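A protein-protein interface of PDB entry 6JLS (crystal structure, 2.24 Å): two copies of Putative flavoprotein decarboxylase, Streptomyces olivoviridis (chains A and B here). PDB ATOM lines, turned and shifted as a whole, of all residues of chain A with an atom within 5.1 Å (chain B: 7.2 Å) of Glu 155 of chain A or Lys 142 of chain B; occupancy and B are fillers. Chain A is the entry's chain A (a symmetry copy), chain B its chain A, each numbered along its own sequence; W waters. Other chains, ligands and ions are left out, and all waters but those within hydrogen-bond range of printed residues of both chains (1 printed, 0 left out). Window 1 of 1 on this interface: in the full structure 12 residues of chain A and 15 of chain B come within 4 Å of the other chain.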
ATOM      1  N   VAL A 122      -0.903   3.250 -14.053  1.00  0.00           N
ATOM      2  CA  VAL A 122      -0.753   3.937 -12.773  1.00  0.00           C
ATOM      3  C   VAL A 122       0.203   5.111 -12.918  1.00  0.00           C
ATOM      4  O   VAL A 122      -0.099   6.233 -12.498  1.00  0.00           O
ATOM      5  CB  VAL A 122      -0.285   2.958 -11.677  1.00  0.00           C
ATOM      6  CG1 VAL A 122       0.074   3.724 -10.370  1.00  0.00           C
ATOM      7  CG2 VAL A 122      -1.357   1.917 -11.406  1.00  0.00           C
ATOM      8  N   MET A 123       1.366   4.878 -13.536  1.00  0.00           N
ATOM      9  CA  MET A 123       2.349   5.954 -13.635  1.00  0.00           C
ATOM     10  C   MET A 123       1.911   7.072 -14.574  1.00  0.00           C
ATOM     11  O   MET A 123       2.453   8.176 -14.482  1.00  0.00           O
ATOM     12  CB  MET A 123       3.703   5.405 -14.068  1.00  0.00           C
ATOM     13  CG  MET A 123       4.389   4.638 -12.967  1.00  0.00           C
ATOM     14  SD  MET A 123       6.099   4.274 -13.361  1.00  0.00           S
ATOM     15  CE  MET A 123       6.764   5.947 -13.429  1.00  0.00           C
ATOM     16  N   ALA A 124       0.944   6.826 -15.464  1.00  0.00           N
ATOM     17  CA  ALA A 124       0.399   7.875 -16.316  1.00  0.00           C
ATOM     18  C   ALA A 124      -0.775   8.605 -15.679  1.00  0.00           C
ATOM     19  O   ALA A 124      -1.176   9.662 -16.174  1.00  0.00           O
ATOM     20  CB  ALA A 124      -0.041   7.293 -17.670  1.00  0.00           C
ATOM     21  N   ALA A 125      -1.330   8.073 -14.601  1.00  0.00           N
ATOM     22  CA  ALA A 125      -2.551   8.618 -14.043  1.00  0.00           C
ATOM     23  C   ALA A 125      -2.256   9.854 -13.208  1.00  0.00           C
ATOM     24  O   ALA A 125      -1.276   9.901 -12.456  1.00  0.00           O
ATOM     25  CB  ALA A 125      -3.264   7.566 -13.192  1.00  0.00           C
ATOM     26  N   ALA A 151       7.819   4.759  -0.666  1.00  0.00           N
ATOM     27  CA  ALA A 151       7.934   5.432  -1.955  1.00  0.00           C
ATOM     28  C   ALA A 151       6.559   5.614  -2.604  1.00  0.00           C
ATOM     29  O   ALA A 151       6.275   6.670  -3.182  1.00  0.00           O
ATOM     30  CB  ALA A 151       8.887   4.646  -2.870  1.00  0.00           C
ATOM     31  N   LEU A 152       5.691   4.600  -2.510  1.00  0.00           N
ATOM     32  CA  LEU A 152       4.374   4.682  -3.140  1.00  0.00           C
ATOM     33  C   LEU A 152       3.557   5.815  -2.548  1.00  0.00           C
ATOM     34  O   LEU A 152       2.796   6.494  -3.247  1.00  0.00           O
ATOM     35  CB  LEU A 152       3.645   3.349  -2.973  1.00  0.00           C
ATOM     36  CG  LEU A 152       4.265   2.284  -3.875  1.00  0.00           C
ATOM     37  CD1 LEU A 152       3.777   0.912  -3.514  1.00  0.00           C
ATOM     38  CD2 LEU A 152       3.980   2.593  -5.335  1.00  0.00           C
ATOM     39  N   ARG A 153       3.742   6.043  -1.278  1.00  0.00           N
ATOM     40  CA  ARG A 153       3.010   7.047  -0.548  1.00  0.00           C
ATOM     41  C   ARG A 153       3.569   8.445  -0.767  1.00  0.00           C
ATOM     42  O   ARG A 153       2.813   9.426  -0.728  1.00  0.00           O
ATOM     43  CB  ARG A 153       3.069   6.640   0.903  1.00  0.00           C
ATOM     44  CG  ARG A 153       2.186   7.306   1.824  1.00  0.00           C
ATOM     45  CD  ARG A 153       2.365   6.507   3.061  1.00  0.00           C
ATOM     46  NE  ARG A 153       1.590   5.274   3.008  1.00  0.00           N
ATOM     47  CZ  ARG A 153       1.889   4.185   3.706  1.00  0.00           C
ATOM     48  NH1 ARG A 153       2.970   4.167   4.462  1.00  0.00           N
ATOM     49  NH2 ARG A 153       1.120   3.106   3.637  1.00  0.00           N
ATOM     50  N   ALA A 154       4.878   8.545  -1.009  1.00  0.00           N
ATOM     51  CA  ALA A 154       5.472   9.783  -1.482  1.00  0.00           C
ATOM     52  C   ALA A 154       4.980  10.160  -2.876  1.00  0.00           C
ATOM     53  O   ALA A 154       4.958  11.350  -3.201  1.00  0.00           O
ATOM     54  CB  ALA A 154       6.997   9.660  -1.470  1.00  0.00           C
ATOM     55  N   GLU A 155       4.606   9.174  -3.711  1.00  0.00           N
ATOM     56  CA  GLU A 155       3.952   9.425  -4.992  1.00  0.00           C
ATOM     57  C   GLU A 155       2.587  10.076  -4.840  1.00  0.00           C
ATOM     58  O   GLU A 155       2.007  10.496  -5.846  1.00  0.00           O
ATOM     59  CB  GLU A 155       3.757   8.121  -5.791  1.00  0.00           C
ATOM     60  CG  GLU A 155       5.024   7.468  -6.260  1.00  0.00           C
ATOM     61  CD  GLU A 155       5.756   8.277  -7.317  1.00  0.00           C
ATOM     62  OE1 GLU A 155       5.096   8.813  -8.227  1.00  0.00           O
ATOM     63  OE2 GLU A 155       6.997   8.384  -7.238  1.00  0.00           O
ATOM     64  N   GLY A 156       2.053  10.154  -3.625  1.00  0.00           N
ATOM     65  CA  GLY A 156       0.697  10.600  -3.426  1.00  0.00           C
ATOM     66  C   GLY A 156      -0.325   9.492  -3.489  1.00  0.00           C
ATOM     67  O   GLY A 156      -1.526   9.771  -3.349  1.00  0.00           O
ATOM     68  N   PHE A 157       0.104   8.248  -3.698  1.00  0.00           N
ATOM     69  CA  PHE A 157      -0.825   7.131  -3.764  1.00  0.00           C
ATOM     70  C   PHE A 157      -1.360   6.805  -2.371  1.00  0.00           C
ATOM     71  O   PHE A 157      -0.677   6.980  -1.358  1.00  0.00           O
ATOM     72  CB  PHE A 157      -0.134   5.889  -4.360  1.00  0.00           C
ATOM     73  CG  PHE A 157       0.410   6.084  -5.760  1.00  0.00           C
ATOM     74  CD1 PHE A 157      -0.041   7.126  -6.573  1.00  0.00           C
ATOM     75  CD2 PHE A 157       1.361   5.205  -6.276  1.00  0.00           C
ATOM     76  CE1 PHE A 157       0.450   7.301  -7.872  1.00  0.00           C
ATOM     77  CE2 PHE A 157       1.859   5.372  -7.585  1.00  0.00           C
ATOM     78  CZ  PHE A 157       1.397   6.428  -8.376  1.00  0.00           C
ATOM     79  N   PRO B 137       5.005  13.933 -19.875  1.00  0.00           N
ATOM     80  CA  PRO B 137       5.338  14.665 -18.639  1.00  0.00           C
ATOM     81  C   PRO B 137       4.467  14.285 -17.439  1.00  0.00           C
ATOM     82  O   PRO B 137       4.793  14.684 -16.320  1.00  0.00           O
ATOM     83  CB  PRO B 137       5.161  16.135 -19.044  1.00  0.00           C
ATOM     84  CG  PRO B 137       5.410  16.133 -20.534  1.00  0.00           C
ATOM     85  CD  PRO B 137       4.791  14.843 -21.014  1.00  0.00           C
ATOM     86  N   ALA B 138       3.394  13.511 -17.630  1.00  0.00           N
ATOM     87  CA  ALA B 138       2.680  12.906 -16.506  1.00  0.00           C
ATOM     88  C   ALA B 138       3.511  11.848 -15.789  1.00  0.00           C
ATOM     89  O   ALA B 138       3.128  11.415 -14.694  1.00  0.00           O
ATOM     90  CB  ALA B 138       1.365  12.282 -16.983  1.00  0.00           C
ATOM     91  N   MET B 139       4.629  11.426 -16.382  1.00  0.00           N
ATOM     92  CA  MET B 139       5.583  10.521 -15.760  1.00  0.00           C
ATOM     93  C   MET B 139       6.880  11.202 -15.344  1.00  0.00           C
ATOM     94  O   MET B 139       7.464  10.822 -14.326  1.00  0.00           O
ATOM     95  CB  MET B 139       5.908   9.361 -16.712  1.00  0.00           C
ATOM     96  CG  MET B 139       4.921   8.217 -16.655  1.00  0.00           C
ATOM     97  SD  MET B 139       5.683   6.627 -17.099  1.00  0.00           S
ATOM     98  CE  MET B 139       5.989   6.849 -18.856  1.00  0.00           C
ATOM     99  N   LEU B 140       7.332  12.217 -16.091  1.00  0.00           N
ATOM    100  CA  LEU B 140       8.655  12.789 -15.864  1.00  0.00           C
ATOM    101  C   LEU B 140       8.728  13.627 -14.592  1.00  0.00           C
ATOM    102  O   LEU B 140       9.832  13.898 -14.103  1.00  0.00           O
ATOM    103  CB  LEU B 140       9.073  13.628 -17.076  1.00  0.00           C
ATOM    104  CG  LEU B 140      10.555  14.018 -17.185  1.00  0.00           C
ATOM    105  CD1 LEU B 140      11.431  12.780 -17.314  1.00  0.00           C
ATOM    106  CD2 LEU B 140      10.807  14.977 -18.340  1.00  0.00           C
ATOM    107  N   ALA B 141       7.589  14.047 -14.046  1.00  0.00           N
ATOM    108  CA  ALA B 141       7.557  14.768 -12.778  1.00  0.00           C
ATOM    109  C   ALA B 141       7.178  13.877 -11.598  1.00  0.00           C
ATOM    110  O   ALA B 141       7.112  14.368 -10.470  1.00  0.00           O
ATOM    111  CB  ALA B 141       6.588  15.951 -12.873  1.00  0.00           C
ATOM    112  N   LYS B 142       6.916  12.590 -11.837  1.00  0.00           N
ATOM    113  CA  LYS B 142       6.653  11.653 -10.756  1.00  0.00           C
ATOM    114  C   LYS B 142       7.896  11.517  -9.876  1.00  0.00           C
ATOM    115  O   LYS B 142       9.009  11.382 -10.395  1.00  0.00           O
ATOM    116  CB  LYS B 142       6.263  10.286 -11.321  1.00  0.00           C
ATOM    117  CG  LYS B 142       4.848  10.176 -11.909  1.00  0.00           C
ATOM    118  CD  LYS B 142       3.926   9.349 -11.002  1.00  0.00           C
ATOM    119  CE  LYS B 142       2.496   9.294 -11.523  1.00  0.00           C
ATOM    120  NZ  LYS B 142       2.031  10.633 -11.980  1.00  0.00           N
ATOM    121  N   PRO B 143       7.743  11.555  -8.546  1.00  0.00           N
ATOM    122  CA  PRO B 143       8.919  11.420  -7.659  1.00  0.00           C
ATOM    123  C   PRO B 143       9.811  10.225  -7.964  1.00  0.00           C
ATOM    124  O   PRO B 143      11.047  10.349  -7.934  1.00  0.00           O
ATOM    125  CB  PRO B 143       8.283  11.295  -6.270  1.00  0.00           C
ATOM    126  CG  PRO B 143       6.981  12.046  -6.388  1.00  0.00           C
ATOM    127  CD  PRO B 143       6.502  11.831  -7.800  1.00  0.00           C
ATOM    128  N   ALA B 144       9.221   9.061  -8.247  1.00  0.00           N
ATOM    129  CA  ALA B 144      10.037   7.872  -8.460  1.00  0.00           C
ATOM    130  C   ALA B 144      10.938   8.039  -9.675  1.00  0.00           C
ATOM    131  O   ALA B 144      12.075   7.550  -9.682  1.00  0.00           O
ATOM    132  CB  ALA B 144       9.153   6.636  -8.606  1.00  0.00           C
ATOM    133  N   VAL B 145      10.461   8.750 -10.703  1.00  0.00           N
ATOM    134  CA  VAL B 145      11.273   8.962 -11.899  1.00  0.00           C
ATOM    135  C   VAL B 145      12.366   9.991 -11.628  1.00  0.00           C
ATOM    136  O   VAL B 145      13.511   9.829 -12.075  1.00  0.00           O
ATOM    137  CB  VAL B 145      10.383   9.370 -13.088  1.00  0.00           C
ATOM    138  CG1 VAL B 145      11.220   9.707 -14.310  1.00  0.00           C
ATOM    139  CG2 VAL B 145       9.437   8.251 -13.431  1.00  0.00           C
ATOM    140  N   ARG B 146      12.033  11.061 -10.889  1.00  0.00           N
ATOM    141  CA  ARG B 146      13.044  12.026 -10.467  1.00  0.00           C
ATOM    142  C   ARG B 146      14.185  11.337  -9.735  1.00  0.00           C
ATOM    143  O   ARG B 146      15.366  11.607 -10.000  1.00  0.00           O
ATOM    144  CB  ARG B 146      12.431  13.082  -9.555  1.00  0.00           C
ATOM    145  CG  ARG B 146      11.333  13.944 -10.127  1.00  0.00           C
ATOM    146  CD  ARG B 146      11.092  15.155  -9.183  1.00  0.00           C
ATOM    147  NE  ARG B 146      10.129  14.929  -8.090  1.00  0.00           N
ATOM    148  CZ  ARG B 146      10.438  14.547  -6.844  1.00  0.00           C
ATOM    149  NH1 ARG B 146      11.699  14.308  -6.487  1.00  0.00           N
ATOM    150  NH2 ARG B 146       9.470  14.391  -5.947  1.00  0.00           N
ATOM    151  N   ARG B 147      13.849  10.457  -8.787  1.00  0.00           N
ATOM    152  CA  ARG B 147      14.889   9.757  -8.042  1.00  0.00           C
ATOM    153  C   ARG B 147      15.705   8.842  -8.946  1.00  0.00           C
ATOM    154  O   ARG B 147      16.920   8.708  -8.761  1.00  0.00           O
ATOM    155  CB  ARG B 147      14.281   8.954  -6.891  1.00  0.00           C
ATOM    156  CG  ARG B 147      13.726   9.797  -5.745  1.00  0.00           C
ATOM    157  CD  ARG B 147      13.510   8.947  -4.490  1.00  0.00           C
ATOM    158  NE  ARG B 147      12.744   7.741  -4.791  1.00  0.00           N
ATOM    159  CZ  ARG B 147      11.416   7.705  -4.805  1.00  0.00           C
ATOM    160  NH1 ARG B 147      10.734   8.804  -4.534  1.00  0.00           N
ATOM    161  NH2 ARG B 147      10.772   6.580  -5.103  1.00  0.00           N
ATOM    162  N   ASN B 148      15.064   8.205  -9.923  1.00  0.00           N
ATOM    163  CA  ASN B 148      15.818   7.372 -10.845  1.00  0.00           C
ATOM    164  C   ASN B 148      16.840   8.201 -11.615  1.00  0.00           C
ATOM    165  O   ASN B 148      17.989   7.776 -11.797  1.00  0.00           O
ATOM    166  CB  ASN B 148      14.859   6.646 -11.789  1.00  0.00           C
ATOM    167  CG  ASN B 148      14.098   5.531 -11.104  1.00  0.00           C
ATOM    168  OD1 ASN B 148      14.522   5.016 -10.069  1.00  0.00           O
ATOM    169  ND2 ASN B 148      12.971   5.140 -11.687  1.00  0.00           N
HETATM  170  O   HOH W   1       8.064   7.623  -4.772  1.00  0.00           O
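No position is printed for both chains.
Water W1 lies within hydrogen-bond range of O of Ala 151 of chain A, OE2 of Glu 155 of chain A and NH2 of Arg 147 of chain B.
Of chain B, only Lys 142 (3.1 Å), Pro 143 (3.3 Å) and Ala 144 (2.5 Å) come within 4 Å of Glu 155 of chain A. Of the printed residues of chain A, Pro 143 of chain B touches Ala 154 and Glu 155. Printed residues of chain B within 4 Å of Ala 154 of chain A: Pro 143 (3.8 Å). Of the printed residues of chain A, Arg 147 of chain B touches Ala 151 (3.5 Å). Of the printed residues of chain A, Ala 138 of chain B touches Met 123 and Ala 124. Printed residues of chain A within 4 Å of Val 145 of chain B: Met 123. Leu 140 of chain B touches none of the printed residues of chain A. Gly 156 of chain A touches none of the printed residues of chain B.
Hydrophobic or aromatic side chains of chain B within 4 Å of the printed part of chain A: Ala 138, Met 139, Pro 143, Ala 144 and Val 145. Printed residues of chain A that touch a printed residue of chain B: Met 123, Ala 124, Ala 125, Ala 151, Ala 154 and Glu 155. Hydrophobic or aromatic side chains of chain A that line the printed part of chain B: Met 123 and Ala 151. Among the printed residues, no Asp or Glu carboxylate lies within 4 Å of a Lys or Arg side-chain nitrogen of the other chain.
O of Ala 138 of chain B lies within hydrogen-bond range of NZ of Lys 142 of chain B (3.0 Å). The side-chain amide nitrogen of Asn 148 of chain B sits close to the backbone carbonyl oxygen of Ala 144 of chain B (3.3 Å).
The side-chain carboxylate (OE2) of Glu 155 of chain A lies within hydrogen-bond range of the backbone NH (N) of Ala 144 of chain B, 2.5 Å away. O of Ala 138 of chain B lies close to O of Met 123 of chain A (3.3 Å). NZ of Lys 142 of chain B lies within hydrogen-bond range of O of Ala 125 of chain A, 3.4 Å away.
Among the printed residues, pairs that only touch across the chains: Glu 155 of chain A with Lys 142 of chain B, Met 123 of chain A with Lys 142 of chain B, Met 123 of chain A with Met 139 of chain B, Glu 155 of chain A with Pro 143 of chain B, Ala 151 of chain A with Arg 147 of chain B, Met 123 of chain A with Val 145 of chain B, Ala 124 of chain A with Ala 138 of chain B and Ala 154 of chain A with Pro 143 of chain B.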
